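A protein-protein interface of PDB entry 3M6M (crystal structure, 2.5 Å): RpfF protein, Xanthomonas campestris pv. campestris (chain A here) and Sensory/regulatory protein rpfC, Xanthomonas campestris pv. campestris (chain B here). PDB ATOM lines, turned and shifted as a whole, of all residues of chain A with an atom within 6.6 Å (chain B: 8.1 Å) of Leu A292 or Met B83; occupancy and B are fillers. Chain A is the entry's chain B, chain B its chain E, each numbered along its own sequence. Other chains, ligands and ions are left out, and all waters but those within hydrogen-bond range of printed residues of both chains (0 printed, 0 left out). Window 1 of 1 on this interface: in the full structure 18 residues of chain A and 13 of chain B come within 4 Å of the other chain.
Of chain B, only Met B83 comes within 4 Å of Leu A292.
Of chain A, only Arg A291 (3.6 Å) and Leu A292 (3.8 Å) come within 4 Å of Met B83.
Of the printed residues of chain A, Gln B79 touches Leu A179, Thr A288 and Arg A291.
Of the printed residues of chain A, Ala B85 touches Leu A210 (3.8 Å).
Printed residues of chain A within 4 Å of Lys B78: Leu A179 (3.7 Å).
Printed residues of chain A within 4 Å of Met B88: Ala A295 (3.98 Å).
Gln B84 touches none of the printed residues of chain A.
The nearest residue of chain B that does not touch Leu A292 is Val B82 (4.6 Å).
The nearest printed residue of chain A that does not touch Lys B78 is Leu A210 (5.7 Å).
Ser B86 touches Leu A152 (OG to CD1, 3.7 Å).
Val B82 touches Pro A176 (CG2 to CB, 3.8 Å).
Lys B78 touches Leu A179.
Leu A179 touches Val B82 (CD1 to CG1, 3.7 Å).
Ala B85 touches Leu A210 (CB to CD1, 3.8 Å).
CG2 of Thr A288 touches OE1 of Gln B79 (3.7 Å).
Met B83 touches Arg A291.
Ala A295 touches Gly B87.
Met B88 touches Ala A295 (N to O, 3.98 Å).
CB of Ser B86 touches CG of Gln A296 (3.9 Å).
Hydrophobic or aromatic side chains of chain B that line the printed part of chain A: Ala B55, Val B82, Met B83 and Ala B85.
Among the printed residues, 18 pairs touch across the chains.
Among the printed residues, Asp or Glu carboxylates within 4 Å of a Lys or Arg side-chain nitrogen of the other chain: Arg A291 with Asp B52 (3.99 Å).
The side-chain hydroxyl (OG) of Ser B86 lies within hydrogen-bond range of the backbone carbonyl oxygen (O) of Val B82 (2.8 Å).
The side-chain hydroxyl (OG1) of Thr A288 lies within hydrogen-bond range of the guanidinium group (NH2) of Arg A291, at 3.2 Å.
The backbone NH (N) of Met B88 lies within hydrogen-bond range of the backbone carbonyl oxygen (O) of Met B83, 3.1 Å away.
NH2 of Arg A291 sits close to NE2 of Gln B79 (3.3 Å).
The guanidinium group of Arg A291 lies within salt-bridge range of the side-chain carboxylate of Asp B52 (3.99 Å).
The side-chain amide oxygen of Gln B79 lies close to the backbone carbonyl oxygen of Leu A179 (3.5 Å).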
ATOM      1  N   ARG A  57       4.426 -22.883 -11.146  1.00  0.00           N
ATOM      2  CA  ARG A  57       4.067 -21.471 -11.254  1.00  0.00           C
ATOM      3  C   ARG A  57       5.147 -20.566 -10.672  1.00  0.00           C
ATOM      4  O   ARG A  57       5.518 -20.700  -9.501  1.00  0.00           O
ATOM      5  CB  ARG A  57       2.726 -21.201 -10.570  1.00  0.00           C
ATOM      6  CG  ARG A  57       1.516 -21.482 -11.447  1.00  0.00           C
ATOM      7  CD  ARG A  57       0.207 -21.161 -10.730  1.00  0.00           C
ATOM      8  NE  ARG A  57      -0.420 -22.349 -10.150  1.00  0.00           N
ATOM      9  CZ  ARG A  57      -0.290 -22.740  -8.885  1.00  0.00           C
ATOM     10  NH1 ARG A  57       0.452 -22.045  -8.033  1.00  0.00           N
ATOM     11  NH2 ARG A  57      -0.911 -23.834  -8.469  1.00  0.00           N
ATOM     12  N   LEU A 104      -1.898 -16.804  -6.420  1.00  0.00           N
ATOM     13  CA  LEU A 104      -3.342 -16.656  -6.619  1.00  0.00           C
ATOM     14  C   LEU A 104      -4.142 -17.884  -6.200  1.00  0.00           C
ATOM     15  O   LEU A 104      -5.253 -17.751  -5.685  1.00  0.00           O
ATOM     16  CB  LEU A 104      -3.655 -16.299  -8.075  1.00  0.00           C
ATOM     17  CG  LEU A 104      -2.969 -15.087  -8.709  1.00  0.00           C
ATOM     18  CD1 LEU A 104      -3.419 -14.934 -10.146  1.00  0.00           C
ATOM     19  CD2 LEU A 104      -3.226 -13.802  -7.924  1.00  0.00           C
ATOM     20  N   LEU A 152       5.055  -9.339 -13.167  1.00  0.00           N
ATOM     21  CA  LEU A 152       3.658  -8.937 -12.989  1.00  0.00           C
ATOM     22  C   LEU A 152       3.255  -8.893 -11.519  1.00  0.00           C
ATOM     23  O   LEU A 152       3.647  -9.757 -10.735  1.00  0.00           O
ATOM     24  CB  LEU A 152       2.716  -9.880 -13.749  1.00  0.00           C
ATOM     25  CG  LEU A 152       3.044 -10.282 -15.193  1.00  0.00           C
ATOM     26  CD1 LEU A 152       2.039 -11.305 -15.699  1.00  0.00           C
ATOM     27  CD2 LEU A 152       3.099  -9.088 -16.131  1.00  0.00           C
ATOM     28  N   PRO A 176      -1.593  -6.317 -12.731  1.00  0.00           N
ATOM     29  CA  PRO A 176      -2.882  -6.805 -13.217  1.00  0.00           C
ATOM     30  C   PRO A 176      -3.915  -7.148 -12.134  1.00  0.00           C
ATOM     31  O   PRO A 176      -4.986  -7.657 -12.460  1.00  0.00           O
ATOM     32  CB  PRO A 176      -2.496  -8.068 -13.988  1.00  0.00           C
ATOM     33  CG  PRO A 176      -1.291  -8.582 -13.281  1.00  0.00           C
ATOM     34  CD  PRO A 176      -0.595  -7.401 -12.644  1.00  0.00           C
ATOM     35  N   LEU A 179      -7.666  -6.387 -12.419  1.00  0.00           N
ATOM     36  CA  LEU A 179      -8.462  -7.202 -13.333  1.00  0.00           C
ATOM     37  C   LEU A 179      -9.311  -8.237 -12.595  1.00  0.00           C
ATOM     38  O   LEU A 179     -10.328  -8.695 -13.119  1.00  0.00           O
ATOM     39  CB  LEU A 179      -7.574  -7.854 -14.401  1.00  0.00           C
ATOM     40  CG  LEU A 179      -6.726  -6.879 -15.236  1.00  0.00           C
ATOM     41  CD1 LEU A 179      -5.655  -7.610 -16.030  1.00  0.00           C
ATOM     42  CD2 LEU A 179      -7.587  -6.020 -16.157  1.00  0.00           C
ATOM     43  N   PHE A 180      -8.889  -8.594 -11.382  1.00  0.00           N
ATOM     44  CA  PHE A 180      -9.736  -9.375 -10.473  1.00  0.00           C
ATOM     45  C   PHE A 180     -10.157  -8.565  -9.235  1.00  0.00           C
ATOM     46  O   PHE A 180     -10.345  -9.113  -8.143  1.00  0.00           O
ATOM     47  CB  PHE A 180      -9.114 -10.737 -10.111  1.00  0.00           C
ATOM     48  CG  PHE A 180      -7.685 -10.672  -9.638  1.00  0.00           C
ATOM     49  CD1 PHE A 180      -7.386 -10.436  -8.298  1.00  0.00           C
ATOM     50  CD2 PHE A 180      -6.638 -10.899 -10.526  1.00  0.00           C
ATOM     51  CE1 PHE A 180      -6.061 -10.396  -7.854  1.00  0.00           C
ATOM     52  CE2 PHE A 180      -5.313 -10.862 -10.096  1.00  0.00           C
ATOM     53  CZ  PHE A 180      -5.024 -10.609  -8.755  1.00  0.00           C
ATOM     54  N   LEU A 210      -0.166  -3.547 -19.236  1.00  0.00           N
ATOM     55  CA  LEU A 210       1.221  -3.984 -19.234  1.00  0.00           C
ATOM     56  C   LEU A 210       2.060  -3.021 -20.065  1.00  0.00           C
ATOM     57  O   LEU A 210       1.587  -2.460 -21.055  1.00  0.00           O
ATOM     58  CB  LEU A 210       1.356  -5.418 -19.753  1.00  0.00           C
ATOM     59  CG  LEU A 210       0.665  -6.551 -18.977  1.00  0.00           C
ATOM     60  CD1 LEU A 210       1.172  -7.902 -19.457  1.00  0.00           C
ATOM     61  CD2 LEU A 210       0.851  -6.424 -17.470  1.00  0.00           C
ATOM     62  N   ARG A 287     -13.094 -16.462 -10.099  1.00  0.00           N
ATOM     63  CA  ARG A 287     -13.009 -17.179 -11.372  1.00  0.00           C
ATOM     64  C   ARG A 287     -11.930 -16.599 -12.290  1.00  0.00           C
ATOM     65  O   ARG A 287     -11.217 -17.347 -12.965  1.00  0.00           O
ATOM     66  CB  ARG A 287     -14.367 -17.229 -12.077  1.00  0.00           C
ATOM     67  CG  ARG A 287     -15.253 -18.386 -11.617  1.00  0.00           C
ATOM     68  CD  ARG A 287     -16.402 -18.650 -12.585  1.00  0.00           C
ATOM     69  NE  ARG A 287     -17.569 -17.808 -12.315  1.00  0.00           N
ATOM     70  CZ  ARG A 287     -17.840 -16.659 -12.931  1.00  0.00           C
ATOM     71  NH1 ARG A 287     -17.026 -16.186 -13.870  1.00  0.00           N
ATOM     72  NH2 ARG A 287     -18.931 -15.979 -12.606  1.00  0.00           N
ATOM     73  N   THR A 288     -11.816 -15.271 -12.303  1.00  0.00           N
ATOM     74  CA  THR A 288     -10.739 -14.581 -13.020  1.00  0.00           C
ATOM     75  C   THR A 288      -9.370 -15.050 -12.522  1.00  0.00           C
ATOM     76  O   THR A 288      -8.474 -15.345 -13.320  1.00  0.00           O
ATOM     77  CB  THR A 288     -10.863 -13.040 -12.879  1.00  0.00           C
ATOM     78  OG1 THR A 288     -12.098 -12.600 -13.459  1.00  0.00           O
ATOM     79  CG2 THR A 288      -9.708 -12.322 -13.571  1.00  0.00           C
ATOM     80  N   MET A 289      -9.227 -15.122 -11.198  1.00  0.00           N
ATOM     81  CA  MET A 289      -8.002 -15.597 -10.561  1.00  0.00           C
ATOM     82  C   MET A 289      -7.686 -17.043 -10.942  1.00  0.00           C
ATOM     83  O   MET A 289      -6.531 -17.370 -11.217  1.00  0.00           O
ATOM     84  CB  MET A 289      -8.094 -15.446  -9.038  1.00  0.00           C
ATOM     85  CG  MET A 289      -7.758 -14.056  -8.520  1.00  0.00           C
ATOM     86  SD  MET A 289      -7.903 -13.889  -6.722  1.00  0.00           S
ATOM     87  CE  MET A 289      -9.607 -13.390  -6.570  1.00  0.00           C
ATOM     88  N   ASP A 290      -8.717 -17.890 -10.969  1.00  0.00           N
ATOM     89  CA  ASP A 290      -8.588 -19.296 -11.375  1.00  0.00           C
ATOM     90  C   ASP A 290      -8.075 -19.450 -12.809  1.00  0.00           C
ATOM     91  O   ASP A 290      -7.243 -20.320 -13.084  1.00  0.00           O
ATOM     92  CB  ASP A 290      -9.926 -20.040 -11.221  1.00  0.00           C
ATOM     93  CG  ASP A 290     -10.279 -20.340  -9.769  1.00  0.00           C
ATOM     94  OD1 ASP A 290      -9.381 -20.320  -8.899  1.00  0.00           O
ATOM     95  OD2 ASP A 290     -11.468 -20.608  -9.499  1.00  0.00           O
ATOM     96  N   ARG A 291      -8.578 -18.609 -13.712  1.00  0.00           N
ATOM     97  CA  ARG A 291      -8.145 -18.612 -15.112  1.00  0.00           C
ATOM     98  C   ARG A 291      -6.684 -18.198 -15.268  1.00  0.00           C
ATOM     99  O   ARG A 291      -5.958 -18.764 -16.091  1.00  0.00           O
ATOM    100  CB  ARG A 291      -9.035 -17.709 -15.964  1.00  0.00           C
ATOM    101  CG  ARG A 291     -10.393 -18.309 -16.307  1.00  0.00           C
ATOM    102  CD  ARG A 291     -11.088 -17.527 -17.417  1.00  0.00           C
ATOM    103  NE  ARG A 291     -11.240 -16.109 -17.084  1.00  0.00           N
ATOM    104  CZ  ARG A 291     -12.280 -15.591 -16.433  1.00  0.00           C
ATOM    105  NH1 ARG A 291     -13.283 -16.364 -16.033  1.00  0.00           N
ATOM    106  NH2 ARG A 291     -12.313 -14.289 -16.180  1.00  0.00           N
ATOM    107  N   LEU A 292      -6.264 -17.212 -14.478  1.00  0.00           N
ATOM    108  CA  LEU A 292      -4.866 -16.780 -14.447  1.00  0.00           C
ATOM    109  C   LEU A 292      -3.945 -17.863 -13.889  1.00  0.00           C
ATOM    110  O   LEU A 292      -2.836 -18.045 -14.389  1.00  0.00           O
ATOM    111  CB  LEU A 292      -4.715 -15.477 -13.654  1.00  0.00           C
ATOM    112  CG  LEU A 292      -4.672 -14.133 -14.396  1.00  0.00           C
ATOM    113  CD1 LEU A 292      -5.790 -13.969 -15.418  1.00  0.00           C
ATOM    114  CD2 LEU A 292      -4.698 -12.985 -13.396  1.00  0.00           C
ATOM    115  N   VAL A 293      -4.415 -18.577 -12.865  1.00  0.00           N
ATOM    116  CA  VAL A 293      -3.678 -19.701 -12.272  1.00  0.00           C
ATOM    117  C   VAL A 293      -3.359 -20.770 -13.323  1.00  0.00           C
ATOM    118  O   VAL A 293      -2.229 -21.261 -13.395  1.00  0.00           O
ATOM    119  CB  VAL A 293      -4.449 -20.326 -11.068  1.00  0.00           C
ATOM    120  CG1 VAL A 293      -3.899 -21.706 -10.702  1.00  0.00           C
ATOM    121  CG2 VAL A 293      -4.389 -19.403  -9.861  1.00  0.00           C
ATOM    122  N   ARG A 294      -4.356 -21.107 -14.138  1.00  0.00           N
ATOM    123  CA  ARG A 294      -4.206 -22.111 -15.192  1.00  0.00           C
ATOM    124  C   ARG A 294      -3.258 -21.658 -16.309  1.00  0.00           C
ATOM    125  O   ARG A 294      -2.497 -22.466 -16.846  1.00  0.00           O
ATOM    126  CB  ARG A 294      -5.576 -22.496 -15.760  1.00  0.00           C
ATOM    127  CG  ARG A 294      -5.550 -23.680 -16.725  1.00  0.00           C
ATOM    128  CD  ARG A 294      -6.924 -24.323 -16.885  1.00  0.00           C
ATOM    129  NE  ARG A 294      -7.966 -23.349 -17.209  1.00  0.00           N
ATOM    130  CZ  ARG A 294      -9.232 -23.657 -17.482  1.00  0.00           C
ATOM    131  NH1 ARG A 294      -9.637 -24.924 -17.484  1.00  0.00           N
ATOM    132  NH2 ARG A 294     -10.097 -22.691 -17.760  1.00  0.00           N
ATOM    133  N   ALA A 295      -3.304 -20.371 -16.649  1.00  0.00           N
ATOM    134  CA  ALA A 295      -2.422 -19.800 -17.670  1.00  0.00           C
ATOM    135  C   ALA A 295      -0.980 -19.690 -17.174  1.00  0.00           C
ATOM    136  O   ALA A 295      -0.036 -19.766 -17.964  1.00  0.00           O
ATOM    137  CB  ALA A 295      -2.940 -18.448 -18.124  1.00  0.00           C
ATOM    138  N   GLN A 296      -0.829 -19.511 -15.861  1.00  0.00           N
ATOM    139  CA  GLN A 296       0.473 -19.529 -15.192  1.00  0.00           C
ATOM    140  C   GLN A 296       1.026 -20.949 -15.127  1.00  0.00           C
ATOM    141  O   GLN A 296       1.353 -21.547 -16.157  1.00  0.00           O
ATOM    142  CB  GLN A 296       0.348 -18.974 -13.773  1.00  0.00           C
ATOM    143  CG  GLN A 296       0.151 -17.471 -13.703  1.00  0.00           C
ATOM    144  CD  GLN A 296      -0.021 -16.952 -12.281  1.00  0.00           C
ATOM    145  OE1 GLN A 296      -0.248 -15.757 -12.076  1.00  0.00           O
ATOM    146  NE2 GLN A 296       0.080 -17.843 -11.296  1.00  0.00           N
ATOM    147  N   LEU B  51     -12.849 -16.283 -23.413  1.00  0.00           N
ATOM    148  CA  LEU B  51     -11.685 -16.607 -22.585  1.00  0.00           C
ATOM    149  C   LEU B  51     -11.707 -18.065 -22.126  1.00  0.00           C
ATOM    150  O   LEU B  51     -10.664 -18.719 -22.074  1.00  0.00           O
ATOM    151  CB  LEU B  51     -11.604 -15.676 -21.370  1.00  0.00           C
ATOM    152  CG  LEU B  51     -11.235 -14.210 -21.611  1.00  0.00           C
ATOM    153  CD1 LEU B  51     -11.677 -13.356 -20.438  1.00  0.00           C
ATOM    154  CD2 LEU B  51      -9.744 -14.044 -21.864  1.00  0.00           C
ATOM    155  N   ASP B  52     -12.898 -18.561 -21.797  1.00  0.00           N
ATOM    156  CA  ASP B  52     -13.091 -19.961 -21.415  1.00  0.00           C
ATOM    157  C   ASP B  52     -12.924 -20.899 -22.611  1.00  0.00           C
ATOM    158  O   ASP B  52     -12.535 -22.057 -22.449  1.00  0.00           O
ATOM    159  CB  ASP B  52     -14.469 -20.164 -20.776  1.00  0.00           C
ATOM    160  CG  ASP B  52     -14.614 -19.444 -19.443  1.00  0.00           C
ATOM    161  OD1 ASP B  52     -13.609 -19.309 -18.712  1.00  0.00           O
ATOM    162  OD2 ASP B  52     -15.743 -19.018 -19.123  1.00  0.00           O
ATOM    163  N   MET B  54     -10.847 -20.157 -25.237  1.00  0.00           N
ATOM    164  CA  MET B  54      -9.426 -20.093 -25.587  1.00  0.00           C
ATOM    165  C   MET B  54      -8.557 -21.007 -24.721  1.00  0.00           C
ATOM    166  O   MET B  54      -7.467 -21.410 -25.133  1.00  0.00           O
ATOM    167  CB  MET B  54      -8.917 -18.652 -25.515  1.00  0.00           C
ATOM    168  CG  MET B  54      -9.380 -17.768 -26.668  1.00  0.00           C
ATOM    169  SD  MET B  54      -8.670 -16.109 -26.642  1.00  0.00           S
ATOM    170  CE  MET B  54      -6.952 -16.480 -26.981  1.00  0.00           C
ATOM    171  N   ALA B  55      -9.044 -21.320 -23.522  1.00  0.00           N
ATOM    172  CA  ALA B  55      -8.385 -22.274 -22.634  1.00  0.00           C
ATOM    173  C   ALA B  55      -8.732 -23.714 -23.015  1.00  0.00           C
ATOM    174  O   ALA B  55      -7.954 -24.637 -22.758  1.00  0.00           O
ATOM    175  CB  ALA B  55      -8.761 -21.999 -21.187  1.00  0.00           C
ATOM    176  N   MET B  76     -11.134  -7.540 -21.983  1.00  0.00           N
ATOM    177  CA  MET B  76     -10.717  -8.844 -22.487  1.00  0.00           C
ATOM    178  C   MET B  76      -9.278  -8.790 -22.997  1.00  0.00           C
ATOM    179  O   MET B  76      -8.483  -9.684 -22.710  1.00  0.00           O
ATOM    180  CB  MET B  76     -11.659  -9.310 -23.603  1.00  0.00           C
ATOM    181  CG  MET B  76     -11.494 -10.772 -23.987  1.00  0.00           C
ATOM    182  SD  MET B  76     -12.062 -11.122 -25.660  1.00  0.00           S
ATOM    183  CE  MET B  76     -10.695 -10.500 -26.638  1.00  0.00           C
ATOM    184  N   LEU B  77      -8.960  -7.736 -23.749  1.00  0.00           N
ATOM    185  CA  LEU B  77      -7.606  -7.488 -24.253  1.00  0.00           C
ATOM    186  C   LEU B  77      -6.597  -7.366 -23.119  1.00  0.00           C
ATOM    187  O   LEU B  77      -5.514  -7.950 -23.184  1.00  0.00           O
ATOM    188  CB  LEU B  77      -7.577  -6.214 -25.101  1.00  0.00           C
ATOM    189  CG  LEU B  77      -7.651  -6.266 -26.632  1.00  0.00           C
ATOM    190  CD1 LEU B  77      -8.679  -7.263 -27.153  1.00  0.00           C
ATOM    191  CD2 LEU B  77      -7.944  -4.872 -27.164  1.00  0.00           C
ATOM    192  N   LYS B  78      -6.962  -6.602 -22.088  1.00  0.00           N
ATOM    193  CA  LYS B  78      -6.128  -6.422 -20.899  1.00  0.00           C
ATOM    194  C   LYS B  78      -5.937  -7.740 -20.159  1.00  0.00           C
ATOM    195  O   LYS B  78      -4.848  -8.028 -19.661  1.00  0.00           O
ATOM    196  CB  LYS B  78      -6.739  -5.385 -19.953  1.00  0.00           C
ATOM    197  CG  LYS B  78      -6.531  -3.942 -20.374  1.00  0.00           C
ATOM    198  CD  LYS B  78      -7.231  -2.991 -19.417  1.00  0.00           C
ATOM    199  CE  LYS B  78      -7.070  -1.549 -19.857  1.00  0.00           C
ATOM    200  NZ  LYS B  78      -7.729  -0.611 -18.911  1.00  0.00           N
ATOM    201  N   GLN B  79      -7.001  -8.536 -20.102  1.00  0.00           N
ATOM    202  CA  GLN B  79      -6.968  -9.818 -19.414  1.00  0.00           C
ATOM    203  C   GLN B  79      -6.189 -10.861 -20.219  1.00  0.00           C
ATOM    204  O   GLN B  79      -5.439 -11.646 -19.642  1.00  0.00           O
ATOM    205  CB  GLN B  79      -8.385 -10.299 -19.093  1.00  0.00           C
ATOM    206  CG  GLN B  79      -8.530 -10.884 -17.698  1.00  0.00           C
ATOM    207  CD  GLN B  79      -9.952 -10.815 -17.178  1.00  0.00           C
ATOM    208  OE1 GLN B  79     -10.293  -9.932 -16.392  1.00  0.00           O
ATOM    209  NE2 GLN B  79     -10.791 -11.743 -17.619  1.00  0.00           N
ATOM    210  N   LEU B  80      -6.354 -10.856 -21.542  1.00  0.00           N
ATOM    211  CA  LEU B  80      -5.580 -11.739 -22.419  1.00  0.00           C
ATOM    212  C   LEU B  80      -4.095 -11.393 -22.420  1.00  0.00           C
ATOM    213  O   LEU B  80      -3.245 -12.285 -22.463  1.00  0.00           O
ATOM    214  CB  LEU B  80      -6.115 -11.718 -23.856  1.00  0.00           C
ATOM    215  CG  LEU B  80      -7.131 -12.785 -24.271  1.00  0.00           C
ATOM    216  CD1 LEU B  80      -7.561 -12.562 -25.710  1.00  0.00           C
ATOM    217  CD2 LEU B  80      -6.576 -14.196 -24.096  1.00  0.00           C
ATOM    218  N   ARG B  81      -3.795 -10.096 -22.375  1.00  0.00           N
ATOM    219  CA  ARG B  81      -2.418  -9.611 -22.348  1.00  0.00           C
ATOM    220  C   ARG B  81      -1.623 -10.206 -21.176  1.00  0.00           C
ATOM    221  O   ARG B  81      -0.500 -10.678 -21.367  1.00  0.00           O
ATOM    222  CB  ARG B  81      -2.384  -8.078 -22.310  1.00  0.00           C
ATOM    223  CG  ARG B  81      -0.986  -7.488 -22.192  1.00  0.00           C
ATOM    224  CD  ARG B  81      -0.391  -7.079 -23.529  1.00  0.00           C
ATOM    225  NE  ARG B  81      -0.296  -5.625 -23.625  1.00  0.00           N
ATOM    226  CZ  ARG B  81       0.637  -4.968 -24.307  1.00  0.00           C
ATOM    227  NH1 ARG B  81       1.579  -5.624 -24.974  1.00  0.00           N
ATOM    228  NH2 ARG B  81       0.629  -3.644 -24.317  1.00  0.00           N
ATOM    229  N   VAL B  82      -2.214 -10.187 -19.980  1.00  0.00           N
ATOM    230  CA  VAL B  82      -1.580 -10.766 -18.791  1.00  0.00           C
ATOM    231  C   VAL B  82      -1.457 -12.298 -18.890  1.00  0.00           C
ATOM    232  O   VAL B  82      -0.428 -12.865 -18.513  1.00  0.00           O
ATOM    233  CB  VAL B  82      -2.254 -10.295 -17.451  1.00  0.00           C
ATOM    234  CG1 VAL B  82      -3.756 -10.438 -17.499  1.00  0.00           C
ATOM    235  CG2 VAL B  82      -1.692 -11.039 -16.244  1.00  0.00           C
ATOM    236  N   MET B  83      -2.491 -12.950 -19.422  1.00  0.00           N
ATOM    237  CA  MET B  83      -2.484 -14.405 -19.614  1.00  0.00           C
ATOM    238  C   MET B  83      -1.381 -14.840 -20.577  1.00  0.00           C
ATOM    239  O   MET B  83      -0.676 -15.817 -20.320  1.00  0.00           O
ATOM    240  CB  MET B  83      -3.846 -14.904 -20.103  1.00  0.00           C
ATOM    241  CG  MET B  83      -4.975 -14.726 -19.102  1.00  0.00           C
ATOM    242  SD  MET B  83      -6.579 -15.242 -19.744  1.00  0.00           S
ATOM    243  CE  MET B  83      -6.697 -16.890 -19.046  1.00  0.00           C
ATOM    244  N   GLN B  84      -1.235 -14.099 -21.675  1.00  0.00           N
ATOM    245  CA  GLN B  84      -0.182 -14.344 -22.660  1.00  0.00           C
ATOM    246  C   GLN B  84       1.210 -14.076 -22.089  1.00  0.00           C
ATOM    247  O   GLN B  84       2.178 -14.744 -22.460  1.00  0.00           O
ATOM    248  CB  GLN B  84      -0.413 -13.504 -23.917  1.00  0.00           C
ATOM    249  CG  GLN B  84      -1.537 -14.018 -24.810  1.00  0.00           C
ATOM    250  CD  GLN B  84      -1.936 -13.036 -25.900  1.00  0.00           C
ATOM    251  OE1 GLN B  84      -1.401 -11.931 -25.992  1.00  0.00           O
ATOM    252  NE2 GLN B  84      -2.885 -13.438 -26.734  1.00  0.00           N
ATOM    253  N   ALA B  85       1.303 -13.104 -21.184  1.00  0.00           N
ATOM    254  CA  ALA B  85       2.552 -12.807 -20.489  1.00  0.00           C
ATOM    255  C   ALA B  85       2.866 -13.859 -19.423  1.00  0.00           C
ATOM    256  O   ALA B  85       4.026 -14.044 -19.047  1.00  0.00           O
ATOM    257  CB  ALA B  85       2.500 -11.421 -19.873  1.00  0.00           C
ATOM    258  N   SER B  86       1.827 -14.542 -18.946  1.00  0.00           N
ATOM    259  CA  SER B  86       1.970 -15.578 -17.921  1.00  0.00           C
ATOM    260  C   SER B  86       2.421 -16.928 -18.484  1.00  0.00           C
ATOM    261  O   SER B  86       3.075 -17.702 -17.784  1.00  0.00           O
ATOM    262  CB  SER B  86       0.670 -15.738 -17.134  1.00  0.00           C
ATOM    263  OG  SER B  86       0.343 -14.542 -16.451  1.00  0.00           O
ATOM    264  N   GLY B  87       2.064 -17.211 -19.736  1.00  0.00           N
ATOM    265  CA  GLY B  87       2.490 -18.446 -20.395  1.00  0.00           C
ATOM    266  C   GLY B  87       1.539 -19.020 -21.432  1.00  0.00           C
ATOM    267  O   GLY B  87       1.821 -20.067 -22.019  1.00  0.00           O
ATOM    268  N   MET B  88       0.415 -18.345 -21.659  1.00  0.00           N
ATOM    269  CA  MET B  88      -0.558 -18.782 -22.655  1.00  0.00           C
ATOM    270  C   MET B  88      -0.048 -18.528 -24.074  1.00  0.00           C
ATOM    271  O   MET B  88       0.706 -17.580 -24.311  1.00  0.00           O
ATOM    272  CB  MET B  88      -1.907 -18.084 -22.445  1.00  0.00           C
ATOM    273  CG  MET B  88      -3.029 -18.602 -23.342  1.00  0.00           C
ATOM    274  SD  MET B  88      -4.326 -17.392 -23.659  1.00  0.00           S
ATOM    275  CE  MET B  88      -5.401 -17.670 -22.263  1.00  0.00           C
ATOM    276  N   ARG B  89      -0.459 -19.394 -25.000  1.00  0.00           N
ATOM    277  CA  ARG B  89      -0.219 -19.218 -26.432  1.00  0.00           C
ATOM    278  C   ARG B  89      -0.750 -17.866 -26.917  1.00  0.00           C
ATOM    279  O   ARG B  89      -1.849 -17.450 -26.541  1.00  0.00           O
ATOM    280  CB  ARG B  89      -0.870 -20.370 -27.213  1.00  0.00           C
ATOM    281  CG  ARG B  89      -1.243 -20.056 -28.663  1.00  0.00           C
ATOM    282  CD  ARG B  89      -1.982 -21.213 -29.322  1.00  0.00           C
ATOM    283  NE  ARG B  89      -1.071 -22.274 -29.747  1.00  0.00           N
ATOM    284  CZ  ARG B  89      -0.521 -22.358 -30.956  1.00  0.00           C
ATOM    285  NH1 ARG B  89      -0.788 -21.443 -31.882  1.00  0.00           N
ATOM    286  NH2 ARG B  89       0.298 -23.362 -31.243  1.00  0.00           N
ATOM    287  N   TYR B  90       0.041 -17.189 -27.745  1.00  0.00           N
ATOM    288  CA  TYR B  90      -0.358 -15.911 -28.327  1.00  0.00           C
ATOM    289  C   TYR B  90      -1.341 -16.093 -29.484  1.00  0.00           C
ATOM    290  O   TYR B  90      -1.127 -16.924 -30.369  1.00  0.00           O
ATOM    291  CB  TYR B  90       0.867 -15.111 -28.793  1.00  0.00           C
ATOM    292  CG  TYR B  90       0.515 -13.795 -29.461  1.00  0.00           C
ATOM    293  CD1 TYR B  90       0.173 -12.676 -28.701  1.00  0.00           C
ATOM    294  CD2 TYR B  90       0.514 -13.673 -30.851  1.00  0.00           C
ATOM    295  CE1 TYR B  90      -0.159 -11.469 -29.305  1.00  0.00           C
ATOM    296  CE2 TYR B  90       0.182 -12.468 -31.467  1.00  0.00           C
ATOM    297  CZ  TYR B  90      -0.153 -11.371 -30.685  1.00  0.00           C
ATOM    298  OH  TYR B  90      -0.481 -10.176 -31.280  1.00  0.00           O
